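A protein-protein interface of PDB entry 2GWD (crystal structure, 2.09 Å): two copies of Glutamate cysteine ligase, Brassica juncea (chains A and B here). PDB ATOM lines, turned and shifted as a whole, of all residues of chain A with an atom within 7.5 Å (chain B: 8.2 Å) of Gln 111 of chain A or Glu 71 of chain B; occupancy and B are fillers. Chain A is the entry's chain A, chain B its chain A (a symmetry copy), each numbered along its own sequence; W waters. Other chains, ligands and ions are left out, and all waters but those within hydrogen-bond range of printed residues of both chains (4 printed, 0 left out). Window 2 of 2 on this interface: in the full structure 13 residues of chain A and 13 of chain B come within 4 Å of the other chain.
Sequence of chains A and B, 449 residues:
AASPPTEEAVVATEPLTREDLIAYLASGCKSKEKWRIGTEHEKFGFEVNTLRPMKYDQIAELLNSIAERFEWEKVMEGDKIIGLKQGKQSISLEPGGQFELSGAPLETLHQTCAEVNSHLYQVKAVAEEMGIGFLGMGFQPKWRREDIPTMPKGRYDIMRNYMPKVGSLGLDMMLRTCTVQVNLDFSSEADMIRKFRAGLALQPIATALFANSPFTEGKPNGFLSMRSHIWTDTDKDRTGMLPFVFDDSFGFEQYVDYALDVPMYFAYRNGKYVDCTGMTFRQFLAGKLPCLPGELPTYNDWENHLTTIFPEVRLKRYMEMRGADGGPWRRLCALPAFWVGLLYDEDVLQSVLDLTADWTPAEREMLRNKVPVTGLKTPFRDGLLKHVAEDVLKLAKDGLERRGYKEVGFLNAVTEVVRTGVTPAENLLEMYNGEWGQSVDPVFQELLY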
ATOM      1  N   ARG A  36     -10.054 -35.503  -1.694  1.00  0.00           N
ATOM      2  CA  ARG A  36     -11.153 -35.127  -0.834  1.00  0.00           C
ATOM      3  C   ARG A  36     -10.674 -34.238   0.329  1.00  0.00           C
ATOM      4  O   ARG A  36      -9.477 -33.981   0.514  1.00  0.00           O
ATOM      5  CB  ARG A  36     -11.839 -36.383  -0.303  1.00  0.00           C
ATOM      6  CG  ARG A  36     -12.474 -37.303  -1.375  1.00  0.00           C
ATOM      7  CD  ARG A  36     -13.690 -36.651  -2.017  1.00  0.00           C
ATOM      8  NE  ARG A  36     -14.319 -37.481  -3.046  1.00  0.00           N
ATOM      9  CZ  ARG A  36     -14.036 -37.428  -4.345  1.00  0.00           C
ATOM     10  NH1 ARG A  36     -13.115 -36.592  -4.808  1.00  0.00           N
ATOM     11  NH2 ARG A  36     -14.677 -38.217  -5.195  1.00  0.00           N
ATOM     12  N   ILE A  37     -11.634 -33.753   1.094  1.00  0.00           N
ATOM     13  CA  ILE A  37     -11.390 -32.818   2.185  1.00  0.00           C
ATOM     14  C   ILE A  37     -11.938 -33.472   3.458  1.00  0.00           C
ATOM     15  O   ILE A  37     -13.134 -33.719   3.555  1.00  0.00           O
ATOM     16  CB  ILE A  37     -12.137 -31.469   1.908  1.00  0.00           C
ATOM     17  CG1 ILE A  37     -11.829 -30.992   0.467  1.00  0.00           C
ATOM     18  CG2 ILE A  37     -11.798 -30.412   2.947  1.00  0.00           C
ATOM     19  CD1 ILE A  37     -12.763 -29.944  -0.062  1.00  0.00           C
ATOM     20  N   PRO A 105     -14.502 -37.946   4.052  1.00  0.00           N
ATOM     21  CA  PRO A 105     -13.754 -37.322   2.948  1.00  0.00           C
ATOM     22  C   PRO A 105     -14.737 -36.748   1.940  1.00  0.00           C
ATOM     23  O   PRO A 105     -15.429 -37.481   1.258  1.00  0.00           O
ATOM     24  CB  PRO A 105     -12.908 -38.463   2.357  1.00  0.00           C
ATOM     25  CG  PRO A 105     -13.329 -39.742   3.071  1.00  0.00           C
ATOM     26  CD  PRO A 105     -14.490 -39.425   3.998  1.00  0.00           C
ATOM     27  N   LEU A 106     -14.795 -35.421   1.864  1.00  0.00           N
ATOM     28  CA  LEU A 106     -15.820 -34.774   1.091  1.00  0.00           C
ATOM     29  C   LEU A 106     -15.208 -34.063  -0.099  1.00  0.00           C
ATOM     30  O   LEU A 106     -14.028 -33.681  -0.081  1.00  0.00           O
ATOM     31  CB  LEU A 106     -16.595 -33.803   1.961  1.00  0.00           C
ATOM     32  CG  LEU A 106     -17.367 -34.443   3.122  1.00  0.00           C
ATOM     33  CD1 LEU A 106     -17.867 -33.343   4.048  1.00  0.00           C
ATOM     34  CD2 LEU A 106     -18.535 -35.298   2.645  1.00  0.00           C
ATOM     35  N   GLU A 107     -16.044 -33.869  -1.118  1.00  0.00           N
ATOM     36  CA  GLU A 107     -15.609 -33.300  -2.378  1.00  0.00           C
ATOM     37  C   GLU A 107     -15.582 -31.760  -2.367  1.00  0.00           C
ATOM     38  O   GLU A 107     -14.670 -31.153  -2.929  1.00  0.00           O
ATOM     39  CB  GLU A 107     -16.486 -33.847  -3.492  1.00  0.00           C
ATOM     40  CG  GLU A 107     -16.172 -33.308  -4.847  1.00  0.00           C
ATOM     41  CD  GLU A 107     -16.766 -34.142  -5.964  1.00  0.00           C
ATOM     42  OE1 GLU A 107     -17.595 -35.061  -5.686  1.00  0.00           O
ATOM     43  OE2 GLU A 107     -16.389 -33.868  -7.128  1.00  0.00           O
ATOM     44  N   THR A 108     -16.560 -31.137  -1.714  1.00  0.00           N
ATOM     45  CA  THR A 108     -16.668 -29.674  -1.692  1.00  0.00           C
ATOM     46  C   THR A 108     -16.831 -29.178  -0.271  1.00  0.00           C
ATOM     47  O   THR A 108     -17.198 -29.929   0.649  1.00  0.00           O
ATOM     48  CB  THR A 108     -17.847 -29.115  -2.565  1.00  0.00           C
ATOM     49  OG1 THR A 108     -19.079 -29.161  -1.852  1.00  0.00           O
ATOM     50  CG2 THR A 108     -17.986 -29.882  -3.862  1.00  0.00           C
ATOM     51  N   LEU A 109     -16.568 -27.889  -0.130  1.00  0.00           N
ATOM     52  CA  LEU A 109     -16.633 -27.197   1.134  1.00  0.00           C
ATOM     53  C   LEU A 109     -18.057 -26.872   1.539  1.00  0.00           C
ATOM     54  O   LEU A 109     -18.311 -26.626   2.710  1.00  0.00           O
ATOM     55  CB  LEU A 109     -15.771 -25.921   1.076  1.00  0.00           C
ATOM     56  CG  LEU A 109     -14.268 -26.189   0.935  1.00  0.00           C
ATOM     57  CD1 LEU A 109     -13.563 -25.023   0.274  1.00  0.00           C
ATOM     58  CD2 LEU A 109     -13.629 -26.445   2.309  1.00  0.00           C
ATOM     59  N   HIS A 110     -18.980 -26.864   0.576  1.00  0.00           N
ATOM     60  CA  HIS A 110     -20.403 -26.790   0.886  1.00  0.00           C
ATOM     61  C   HIS A 110     -20.802 -28.019   1.689  1.00  0.00           C
ATOM     62  O   HIS A 110     -21.509 -27.910   2.681  1.00  0.00           O
ATOM     63  CB  HIS A 110     -21.272 -26.653  -0.383  1.00  0.00           C
ATOM     64  CG  HIS A 110     -20.910 -25.468  -1.230  1.00  0.00           C
ATOM     65  ND1 HIS A 110     -21.090 -24.168  -0.805  1.00  0.00           N
ATOM     66  CD2 HIS A 110     -20.358 -25.389  -2.465  1.00  0.00           C
ATOM     67  CE1 HIS A 110     -20.659 -23.342  -1.738  1.00  0.00           C
ATOM     68  NE2 HIS A 110     -20.219 -24.058  -2.761  1.00  0.00           N
ATOM     69  N   GLN A 111     -20.318 -29.176   1.259  1.00  0.00           N
ATOM     70  CA  GLN A 111     -20.534 -30.430   1.970  1.00  0.00           C
ATOM     71  C   GLN A 111     -19.854 -30.390   3.333  1.00  0.00           C
ATOM     72  O   GLN A 111     -20.429 -30.829   4.320  1.00  0.00           O
ATOM     73  CB  GLN A 111     -20.032 -31.631   1.154  1.00  0.00           C
ATOM     74  CG  GLN A 111     -20.770 -31.846  -0.169  1.00  0.00           C
ATOM     75  CD  GLN A 111     -19.986 -32.733  -1.138  1.00  0.00           C
ATOM     76  OE1 GLN A 111     -18.772 -32.958  -0.962  1.00  0.00           O
ATOM     77  NE2 GLN A 111     -20.677 -33.247  -2.162  1.00  0.00           N
ATOM     78  N   THR A 112     -18.625 -29.873   3.392  1.00  0.00           N
ATOM     79  CA  THR A 112     -17.938 -29.725   4.673  1.00  0.00           C
ATOM     80  C   THR A 112     -18.787 -28.937   5.699  1.00  0.00           C
ATOM     81  O   THR A 112     -18.998 -29.379   6.832  1.00  0.00           O
ATOM     82  CB  THR A 112     -16.569 -29.010   4.468  1.00  0.00           C
ATOM     83  OG1 THR A 112     -15.739 -29.793   3.601  1.00  0.00           O
ATOM     84  CG2 THR A 112     -15.861 -28.789   5.786  1.00  0.00           C
ATOM     85  N   CYS A 113     -19.276 -27.768   5.286  1.00  0.00           N
ATOM     86  CA  CYS A 113     -19.980 -26.898   6.198  1.00  0.00           C
ATOM     87  C   CYS A 113     -21.364 -27.444   6.601  1.00  0.00           C
ATOM     88  O   CYS A 113     -21.781 -27.279   7.747  1.00  0.00           O
ATOM     89  CB  CYS A 113     -20.072 -25.482   5.625  1.00  0.00           C
ATOM     90  SG  CYS A 113     -20.226 -24.221   6.945  1.00  0.00           S
ATOM     91  N   ALA A 114     -22.067 -28.065   5.652  1.00  0.00           N
ATOM     92  CA  ALA A 114     -23.248 -28.851   5.939  1.00  0.00           C
ATOM     93  C   ALA A 114     -22.951 -29.943   6.964  1.00  0.00           C
ATOM     94  O   ALA A 114     -23.731 -30.181   7.861  1.00  0.00           O
ATOM     95  CB  ALA A 114     -23.794 -29.469   4.659  1.00  0.00           C
ATOM     96  N   GLU A 115     -21.808 -30.608   6.829  1.00  0.00           N
ATOM     97  CA  GLU A 115     -21.424 -31.631   7.791  1.00  0.00           C
ATOM     98  C   GLU A 115     -21.185 -31.028   9.178  1.00  0.00           C
ATOM     99  O   GLU A 115     -21.562 -31.605  10.173  1.00  0.00           O
ATOM    100  CB  GLU A 115     -20.165 -32.348   7.314  1.00  0.00           C
ATOM    101  CG  GLU A 115     -19.795 -33.546   8.138  1.00  0.00           C
ATOM    102  CD  GLU A 115     -18.453 -34.091   7.725  1.00  0.00           C
ATOM    103  OE1 GLU A 115     -17.439 -33.361   7.875  1.00  0.00           O
ATOM    104  OE2 GLU A 115     -18.422 -35.234   7.250  1.00  0.00           O
ATOM    105  N   VAL A 116     -20.539 -29.867   9.243  1.00  0.00           N
ATOM    106  CA  VAL A 116     -20.300 -29.208  10.532  1.00  0.00           C
ATOM    107  C   VAL A 116     -21.670 -28.880  11.171  1.00  0.00           C
ATOM    108  O   VAL A 116     -21.913 -29.197  12.324  1.00  0.00           O
ATOM    109  CB  VAL A 116     -19.405 -27.958  10.361  1.00  0.00           C
ATOM    110  CG1 VAL A 116     -19.429 -27.051  11.607  1.00  0.00           C
ATOM    111  CG2 VAL A 116     -17.972 -28.372  10.054  1.00  0.00           C
ATOM    112  N   ASN A 117     -22.581 -28.308  10.391  1.00  0.00           N
ATOM    113  CA  ASN A 117     -23.897 -27.929  10.888  1.00  0.00           C
ATOM    114  C   ASN A 117     -24.707 -29.120  11.411  1.00  0.00           C
ATOM    115  O   ASN A 117     -25.347 -29.044  12.464  1.00  0.00           O
ATOM    116  CB  ASN A 117     -24.687 -27.185   9.817  1.00  0.00           C
ATOM    117  CG  ASN A 117     -26.096 -26.928  10.239  1.00  0.00           C
ATOM    118  OD1 ASN A 117     -26.997 -27.716   9.931  1.00  0.00           O
ATOM    119  ND2 ASN A 117     -26.307 -25.838  10.981  1.00  0.00           N
ATOM    120  N   ARG A 403     -11.601 -23.602  -8.645  1.00  0.00           N
ATOM    121  CA  ARG A 403     -12.282 -24.889  -8.436  1.00  0.00           C
ATOM    122  C   ARG A 403     -13.684 -24.954  -9.051  1.00  0.00           C
ATOM    123  O   ARG A 403     -14.163 -26.037  -9.329  1.00  0.00           O
ATOM    124  CB  ARG A 403     -12.341 -25.257  -6.951  1.00  0.00           C
ATOM    125  CG  ARG A 403     -11.089 -25.929  -6.450  1.00  0.00           C
ATOM    126  CD  ARG A 403     -11.063 -26.121  -4.943  1.00  0.00           C
ATOM    127  NE  ARG A 403     -12.226 -26.827  -4.393  1.00  0.00           N
ATOM    128  CZ  ARG A 403     -12.339 -28.146  -4.186  1.00  0.00           C
ATOM    129  NH1 ARG A 403     -11.399 -29.001  -4.548  1.00  0.00           N
ATOM    130  NH2 ARG A 403     -13.445 -28.620  -3.643  1.00  0.00           N
ATOM    131  N   GLU A 407     -17.053 -21.733  -3.725  1.00  0.00           N
ATOM    132  CA  GLU A 407     -16.699 -21.948  -2.329  1.00  0.00           C
ATOM    133  C   GLU A 407     -16.048 -20.735  -1.663  1.00  0.00           C
ATOM    134  O   GLU A 407     -15.731 -20.784  -0.471  1.00  0.00           O
ATOM    135  CB  GLU A 407     -15.761 -23.150  -2.195  1.00  0.00           C
ATOM    136  CG  GLU A 407     -16.350 -24.482  -2.599  1.00  0.00           C
ATOM    137  CD  GLU A 407     -15.275 -25.503  -2.932  1.00  0.00           C
ATOM    138  OE1 GLU A 407     -14.411 -25.164  -3.760  1.00  0.00           O
ATOM    139  OE2 GLU A 407     -15.308 -26.642  -2.404  1.00  0.00           O
ATOM    140  N   PHE A 410     -16.612 -18.967   1.935  1.00  0.00           N
ATOM    141  CA  PHE A 410     -16.090 -19.583   3.175  1.00  0.00           C
ATOM    142  C   PHE A 410     -14.870 -18.885   3.760  1.00  0.00           C
ATOM    143  O   PHE A 410     -14.535 -19.102   4.911  1.00  0.00           O
ATOM    144  CB  PHE A 410     -15.821 -21.089   2.990  1.00  0.00           C
ATOM    145  CG  PHE A 410     -17.085 -21.896   2.866  1.00  0.00           C
ATOM    146  CD1 PHE A 410     -17.980 -21.958   3.933  1.00  0.00           C
ATOM    147  CD2 PHE A 410     -17.432 -22.508   1.674  1.00  0.00           C
ATOM    148  CE1 PHE A 410     -19.165 -22.647   3.821  1.00  0.00           C
ATOM    149  CE2 PHE A 410     -18.618 -23.229   1.570  1.00  0.00           C
ATOM    150  CZ  PHE A 410     -19.481 -23.295   2.649  1.00  0.00           C
ATOM    151  N   ASN B  64     -31.598 -23.009  -7.797  1.00  0.00           N
ATOM    152  CA  ASN B  64     -30.423 -23.466  -8.605  1.00  0.00           C
ATOM    153  C   ASN B  64     -29.143 -23.706  -7.777  1.00  0.00           C
ATOM    154  O   ASN B  64     -28.385 -24.646  -8.015  1.00  0.00           O
ATOM    155  CB  ASN B  64     -30.066 -22.458  -9.693  1.00  0.00           C
ATOM    156  CG  ASN B  64     -31.057 -22.448 -10.874  1.00  0.00           C
ATOM    157  OD1 ASN B  64     -31.432 -21.377 -11.375  1.00  0.00           O
ATOM    158  ND2 ASN B  64     -31.459 -23.618 -11.332  1.00  0.00           N
ATOM    159  N   SER B  65     -28.902 -22.798  -6.837  1.00  0.00           N
ATOM    160  CA  SER B  65     -27.737 -22.846  -5.979  1.00  0.00           C
ATOM    161  C   SER B  65     -27.841 -24.003  -4.989  1.00  0.00           C
ATOM    162  O   SER B  65     -26.874 -24.728  -4.802  1.00  0.00           O
ATOM    163  CB  SER B  65     -27.593 -21.512  -5.240  1.00  0.00           C
ATOM    164  OG  SER B  65     -27.100 -20.507  -6.102  1.00  0.00           O
ATOM    165  N   ILE B  66     -29.005 -24.179  -4.354  1.00  0.00           N
ATOM    166  CA  ILE B  66     -29.233 -25.346  -3.472  1.00  0.00           C
ATOM    167  C   ILE B  66     -29.042 -26.672  -4.218  1.00  0.00           C
ATOM    168  O   ILE B  66     -28.523 -27.644  -3.636  1.00  0.00           O
ATOM    169  CB  ILE B  66     -30.664 -25.340  -2.823  1.00  0.00           C
ATOM    170  CG1 ILE B  66     -30.802 -24.216  -1.804  1.00  0.00           C
ATOM    171  CG2 ILE B  66     -30.985 -26.675  -2.151  1.00  0.00           C
ATOM    172  CD1 ILE B  66     -32.236 -23.935  -1.457  1.00  0.00           C
ATOM    173  N   ALA B  67     -29.473 -26.705  -5.484  1.00  0.00           N
ATOM    174  CA  ALA B  67     -29.416 -27.899  -6.295  1.00  0.00           C
ATOM    175  C   ALA B  67     -27.977 -28.289  -6.562  1.00  0.00           C
ATOM    176  O   ALA B  67     -27.620 -29.456  -6.484  1.00  0.00           O
ATOM    177  CB  ALA B  67     -30.158 -27.693  -7.627  1.00  0.00           C
ATOM    178  N   GLU B  68     -27.171 -27.293  -6.912  1.00  0.00           N
ATOM    179  CA  GLU B  68     -25.778 -27.499  -7.232  1.00  0.00           C
ATOM    180  C   GLU B  68     -24.951 -27.810  -5.983  1.00  0.00           C
ATOM    181  O   GLU B  68     -24.118 -28.721  -6.004  1.00  0.00           O
ATOM    182  CB  GLU B  68     -25.216 -26.250  -7.917  1.00  0.00           C
ATOM    183  CG  GLU B  68     -23.828 -26.431  -8.451  1.00  0.00           C
ATOM    184  CD  GLU B  68     -23.188 -25.118  -8.946  1.00  0.00           C
ATOM    185  OE1 GLU B  68     -23.870 -24.062  -8.868  1.00  0.00           O
ATOM    186  OE2 GLU B  68     -22.005 -25.165  -9.385  1.00  0.00           O
ATOM    187  N   ARG B  69     -25.159 -27.039  -4.915  1.00  0.00           N
ATOM    188  CA  ARG B  69     -24.348 -27.198  -3.703  1.00  0.00           C
ATOM    189  C   ARG B  69     -24.634 -28.481  -2.926  1.00  0.00           C
ATOM    190  O   ARG B  69     -23.710 -29.113  -2.403  1.00  0.00           O
ATOM    191  CB  ARG B  69     -24.542 -26.009  -2.768  1.00  0.00           C
ATOM    192  CG  ARG B  69     -23.998 -24.750  -3.334  1.00  0.00           C
ATOM    193  CD  ARG B  69     -24.246 -23.625  -2.368  1.00  0.00           C
ATOM    194  NE  ARG B  69     -23.835 -22.366  -2.942  1.00  0.00           N
ATOM    195  CZ  ARG B  69     -23.602 -21.258  -2.249  1.00  0.00           C
ATOM    196  NH1 ARG B  69     -23.674 -21.231  -0.927  1.00  0.00           N
ATOM    197  NH2 ARG B  69     -23.235 -20.181  -2.899  1.00  0.00           N
ATOM    198  N   PHE B  70     -25.913 -28.848  -2.869  1.00  0.00           N
ATOM    199  CA  PHE B  70     -26.394 -29.874  -1.963  1.00  0.00           C
ATOM    200  C   PHE B  70     -27.049 -31.053  -2.684  1.00  0.00           C
ATOM    201  O   PHE B  70     -27.709 -31.868  -2.054  1.00  0.00           O
ATOM    202  CB  PHE B  70     -27.361 -29.245  -0.961  1.00  0.00           C
ATOM    203  CG  PHE B  70     -26.756 -28.105  -0.186  1.00  0.00           C
ATOM    204  CD1 PHE B  70     -25.634 -28.315   0.608  1.00  0.00           C
ATOM    205  CD2 PHE B  70     -27.279 -26.824  -0.269  1.00  0.00           C
ATOM    206  CE1 PHE B  70     -25.048 -27.259   1.309  1.00  0.00           C
ATOM    207  CE2 PHE B  70     -26.690 -25.767   0.441  1.00  0.00           C
ATOM    208  CZ  PHE B  70     -25.575 -26.000   1.228  1.00  0.00           C
ATOM    209  N   GLU B  71     -26.854 -31.124  -4.001  1.00  0.00           N
ATOM    210  CA  GLU B  71     -27.248 -32.255  -4.822  1.00  0.00           C
ATOM    211  C   GLU B  71     -28.743 -32.547  -4.802  1.00  0.00           C
ATOM    212  O   GLU B  71     -29.176 -33.595  -4.343  1.00  0.00           O
ATOM    213  CB  GLU B  71     -26.426 -33.504  -4.455  1.00  0.00           C
ATOM    214  CG  GLU B  71     -24.969 -33.343  -4.822  1.00  0.00           C
ATOM    215  CD  GLU B  71     -24.126 -34.565  -4.473  1.00  0.00           C
ATOM    216  OE1 GLU B  71     -24.020 -35.495  -5.324  1.00  0.00           O
ATOM    217  OE2 GLU B  71     -23.562 -34.568  -3.353  1.00  0.00           O
ATOM    218  N   TRP B  72     -29.517 -31.596  -5.307  1.00  0.00           N
ATOM    219  CA  TRP B  72     -30.951 -31.789  -5.538  1.00  0.00           C
ATOM    220  C   TRP B  72     -31.202 -31.818  -7.057  1.00  0.00           C
ATOM    221  O   TRP B  72     -30.497 -31.181  -7.842  1.00  0.00           O
ATOM    222  CB  TRP B  72     -31.778 -30.668  -4.940  1.00  0.00           C
ATOM    223  CG  TRP B  72     -31.789 -30.608  -3.465  1.00  0.00           C
ATOM    224  CD1 TRP B  72     -30.765 -30.221  -2.652  1.00  0.00           C
ATOM    225  CD2 TRP B  72     -32.889 -30.901  -2.608  1.00  0.00           C
ATOM    226  NE1 TRP B  72     -31.153 -30.273  -1.340  1.00  0.00           N
ATOM    227  CE2 TRP B  72     -32.456 -30.691  -1.284  1.00  0.00           C
ATOM    228  CE3 TRP B  72     -34.205 -31.333  -2.829  1.00  0.00           C
ATOM    229  CZ2 TRP B  72     -33.293 -30.898  -0.184  1.00  0.00           C
ATOM    230  CZ3 TRP B  72     -35.025 -31.540  -1.735  1.00  0.00           C
ATOM    231  CH2 TRP B  72     -34.576 -31.316  -0.439  1.00  0.00           C
ATOM    232  N   GLU B  73     -32.209 -32.575  -7.445  1.00  0.00           N
ATOM    233  CA  GLU B  73     -32.690 -32.638  -8.810  1.00  0.00           C
ATOM    234  C   GLU B  73     -33.642 -31.461  -9.028  1.00  0.00           C
ATOM    235  O   GLU B  73     -34.448 -31.140  -8.167  1.00  0.00           O
ATOM    236  CB  GLU B  73     -33.397 -33.981  -8.997  1.00  0.00           C
ATOM    237  CG  GLU B  73     -33.978 -34.278 -10.376  1.00  0.00           C
ATOM    238  CD  GLU B  73     -34.753 -35.617 -10.373  1.00  0.00           C
ATOM    239  OE1 GLU B  73     -34.072 -36.674 -10.323  1.00  0.00           O
ATOM    240  OE2 GLU B  73     -36.016 -35.609 -10.369  1.00  0.00           O
ATOM    241  N   LYS B  74     -33.525 -30.803 -10.174  1.00  0.00           N
ATOM    242  CA  LYS B  74     -34.385 -29.662 -10.518  1.00  0.00           C
ATOM    243  C   LYS B  74     -35.770 -30.081 -11.037  1.00  0.00           C
ATOM    244  O   LYS B  74     -35.893 -31.011 -11.817  1.00  0.00           O
ATOM    245  CB  LYS B  74     -33.697 -28.790 -11.583  1.00  0.00           C
ATOM    246  CG  LYS B  74     -32.328 -28.261 -11.137  1.00  0.00           C
ATOM    247  CD  LYS B  74     -31.694 -27.384 -12.175  1.00  0.00           C
ATOM    248  CE  LYS B  74     -30.397 -26.819 -11.670  1.00  0.00           C
ATOM    249  NZ  LYS B  74     -29.566 -26.267 -12.788  1.00  0.00           N
ATOM    250  N   LEU B  84     -37.369 -28.559  -6.346  1.00  0.00           N
ATOM    251  CA  LEU B  84     -36.234 -29.486  -6.259  1.00  0.00           C
ATOM    252  C   LEU B  84     -36.694 -30.825  -5.649  1.00  0.00           C
ATOM    253  O   LEU B  84     -37.655 -30.855  -4.890  1.00  0.00           O
ATOM    254  CB  LEU B  84     -35.142 -28.910  -5.386  1.00  0.00           C
ATOM    255  CG  LEU B  84     -34.466 -27.604  -5.828  1.00  0.00           C
ATOM    256  CD1 LEU B  84     -33.600 -27.072  -4.694  1.00  0.00           C
ATOM    257  CD2 LEU B  84     -33.645 -27.844  -7.065  1.00  0.00           C
ATOM    258  N   LYS B  85     -35.997 -31.900  -5.997  1.00  0.00           N
ATOM    259  CA  LYS B  85     -36.269 -33.243  -5.473  1.00  0.00           C
ATOM    260  C   LYS B  85     -34.982 -33.871  -4.977  1.00  0.00           C
ATOM    261  O   LYS B  85     -33.959 -33.761  -5.630  1.00  0.00           O
ATOM    262  CB  LYS B  85     -36.852 -34.147  -6.578  1.00  0.00           C
ATOM    263  CG  LYS B  85     -38.351 -33.955  -6.791  1.00  0.00           C
ATOM    264  CD  LYS B  85     -38.865 -34.761  -8.012  1.00  0.00           C
ATOM    265  CE  LYS B  85     -39.548 -36.058  -7.591  1.00  0.00           C
ATOM    266  NZ  LYS B  85     -38.638 -37.160  -7.158  1.00  0.00           N
ATOM    267  N   GLN B  86     -35.047 -34.555  -3.842  1.00  0.00           N
ATOM    268  CA  GLN B  86     -33.923 -35.355  -3.369  1.00  0.00           C
ATOM    269  C   GLN B  86     -34.468 -36.524  -2.561  1.00  0.00           C
ATOM    270  O   GLN B  86     -35.009 -36.338  -1.464  1.00  0.00           O
ATOM    271  CB  GLN B  86     -32.982 -34.507  -2.526  1.00  0.00           C
ATOM    272  CG  GLN B  86     -31.679 -35.182  -2.139  1.00  0.00           C
ATOM    273  CD  GLN B  86     -30.946 -34.405  -1.073  1.00  0.00           C
ATOM    274  OE1 GLN B  86     -29.931 -33.760  -1.344  1.00  0.00           O
ATOM    275  NE2 GLN B  86     -31.477 -34.421   0.126  1.00  0.00           N
ATOM    276  N   GLY B  87     -34.343 -37.727  -3.118  1.00  0.00           N
ATOM    277  CA  GLY B  87     -35.057 -38.875  -2.585  1.00  0.00           C
ATOM    278  C   GLY B  87     -36.517 -38.566  -2.393  1.00  0.00           C
ATOM    279  O   GLY B  87     -37.193 -38.140  -3.309  1.00  0.00           O
ATOM    280  N   TYR B 121     -30.564 -24.775   7.201  1.00  0.00           N
ATOM    281  CA  TYR B 121     -29.164 -24.578   6.931  1.00  0.00           C
ATOM    282  C   TYR B 121     -28.913 -24.358   5.425  1.00  0.00           C
ATOM    283  O   TYR B 121     -28.208 -23.438   5.061  1.00  0.00           O
ATOM    284  CB  TYR B 121     -28.284 -25.739   7.433  1.00  0.00           C
ATOM    285  CG  TYR B 121     -26.881 -25.530   6.949  1.00  0.00           C
ATOM    286  CD1 TYR B 121     -26.060 -24.576   7.556  1.00  0.00           C
ATOM    287  CD2 TYR B 121     -26.401 -26.181   5.816  1.00  0.00           C
ATOM    288  CE1 TYR B 121     -24.792 -24.335   7.098  1.00  0.00           C
ATOM    289  CE2 TYR B 121     -25.126 -25.929   5.347  1.00  0.00           C
ATOM    290  CZ  TYR B 121     -24.333 -24.994   6.000  1.00  0.00           C
ATOM    291  OH  TYR B 121     -23.072 -24.699   5.542  1.00  0.00           O
ATOM    292  N   GLN B 122     -29.426 -25.247   4.575  1.00  0.00           N
ATOM    293  CA  GLN B 122     -29.123 -25.168   3.141  1.00  0.00           C
ATOM    294  C   GLN B 122     -29.686 -23.880   2.563  1.00  0.00           C
ATOM    295  O   GLN B 122     -29.010 -23.186   1.802  1.00  0.00           O
ATOM    296  CB  GLN B 122     -29.651 -26.388   2.381  1.00  0.00           C
ATOM    297  CG  GLN B 122     -28.928 -27.645   2.743  1.00  0.00           C
ATOM    298  CD  GLN B 122     -29.386 -28.851   1.950  1.00  0.00           C
ATOM    299  OE1 GLN B 122     -30.222 -28.739   1.045  1.00  0.00           O
ATOM    300  NE2 GLN B 122     -28.840 -30.029   2.297  1.00  0.00           N
HETATM  301  O   HOH W   1     -23.818 -32.021  -1.981  1.00  0.00           O
HETATM  302  O   HOH W   2     -22.913 -23.423   1.115  1.00  0.00           O
HETATM  303  O   HOH W   3     -22.558 -25.255   3.122  1.00  0.00           O
HETATM  304  O   HOH W   4     -21.162 -29.014  -3.252  1.00  0.00           O
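NE2 of Gln 111 of chain A is in hydrogen-bond range of OE2 of Glu 71 of chain B, at 3.4 Å.
The side-chain hydroxyl (OH) of Tyr 121 of chain B sits close to the side-chain sulfur (SG) of Cys 113 of chain A.
The backbone NH (N) of Glu 107 of chain A sits at hydrogen-bond distance from the side-chain amide oxygen (OE1) of Gln 111 of chain A (2.9 Å).
OG1 of Thr 108 of chain A lies close to N of His 110 of chain A (3.3 Å).
O of Phe 70 of chain B lies close to OE1 of Gln 86 of chain B (3.0 Å).
The backbone carbonyl oxygen of Glu 71 of chain B lies close to the side-chain amide oxygen of Gln 86 of chain B (3.1 Å).
Among the printed residues, merely in contact across the chains: Asn 117 of chain A with Tyr 121 of chain B, Ala 114 of chain A with Tyr 121 of chain B, His 110 of chain A with Arg 69 of chain B and His 110 of chain A with Phe 70 of chain B.
Of the printed residues of chain B, His 110 of chain A touches Arg 69 and Phe 70.
Of chain B, only Glu 71 comes within 4 Å of Gln 111 of chain A.
Printed residues of chain B within 4 Å of Asn 117 of chain A: Tyr 121 (3.4 Å).
Of chain A, only Gln 111 (3.4 Å) comes within 4 Å of Glu 71 of chain B.
Lys 85 of chain B touches none of the printed residues of chain A.
Printed residues of chain A within 4 Å of Tyr 121 of chain B: Cys 113 (3.1 Å), Ala 114 (3.5 Å) and Asn 117 (3.4 Å).
Gln 122 of chain B touches none of the printed residues of chain A.
Of the 17 printed residues of chain B, 4 touch a printed residue of chain A.
Hydrophobic or aromatic side chains of chain B within 4 Å of the printed part of chain A: Phe 70 and Tyr 121.
Printed residues of chain A that touch a printed residue of chain B: His 110, Gln 111, Cys 113, Ala 114 and Asn 117.
Among the printed residues, 6 pairs touch across the chains.
Among the printed residues, no Asp or Glu carboxylate lies within 4 Å of a Lys or Arg side-chain nitrogen of the other chain.
No position is printed for both chains.
Of the 6 pairs that touch across the chains among the printed residues, none has its exchanged pair printed and touching as well.
Water W4 lies within hydrogen-bond range of the side-chain hydroxyl of Thr 108 of chain A and the backbone carbonyl oxygen of Arg 69 of chain B.
Water W2 bridges a ring nitrogen (ND1) of His 110 of chain A and the guanidinium group of Arg 69 of chain B.
Water W1 lies within hydrogen-bond range of OE2 of Glu 71 of chain B (2.9 Å), O of Arg 69 of chain B (2.9 Å) and NE2 of Gln 111 of chain A (3.4 Å).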
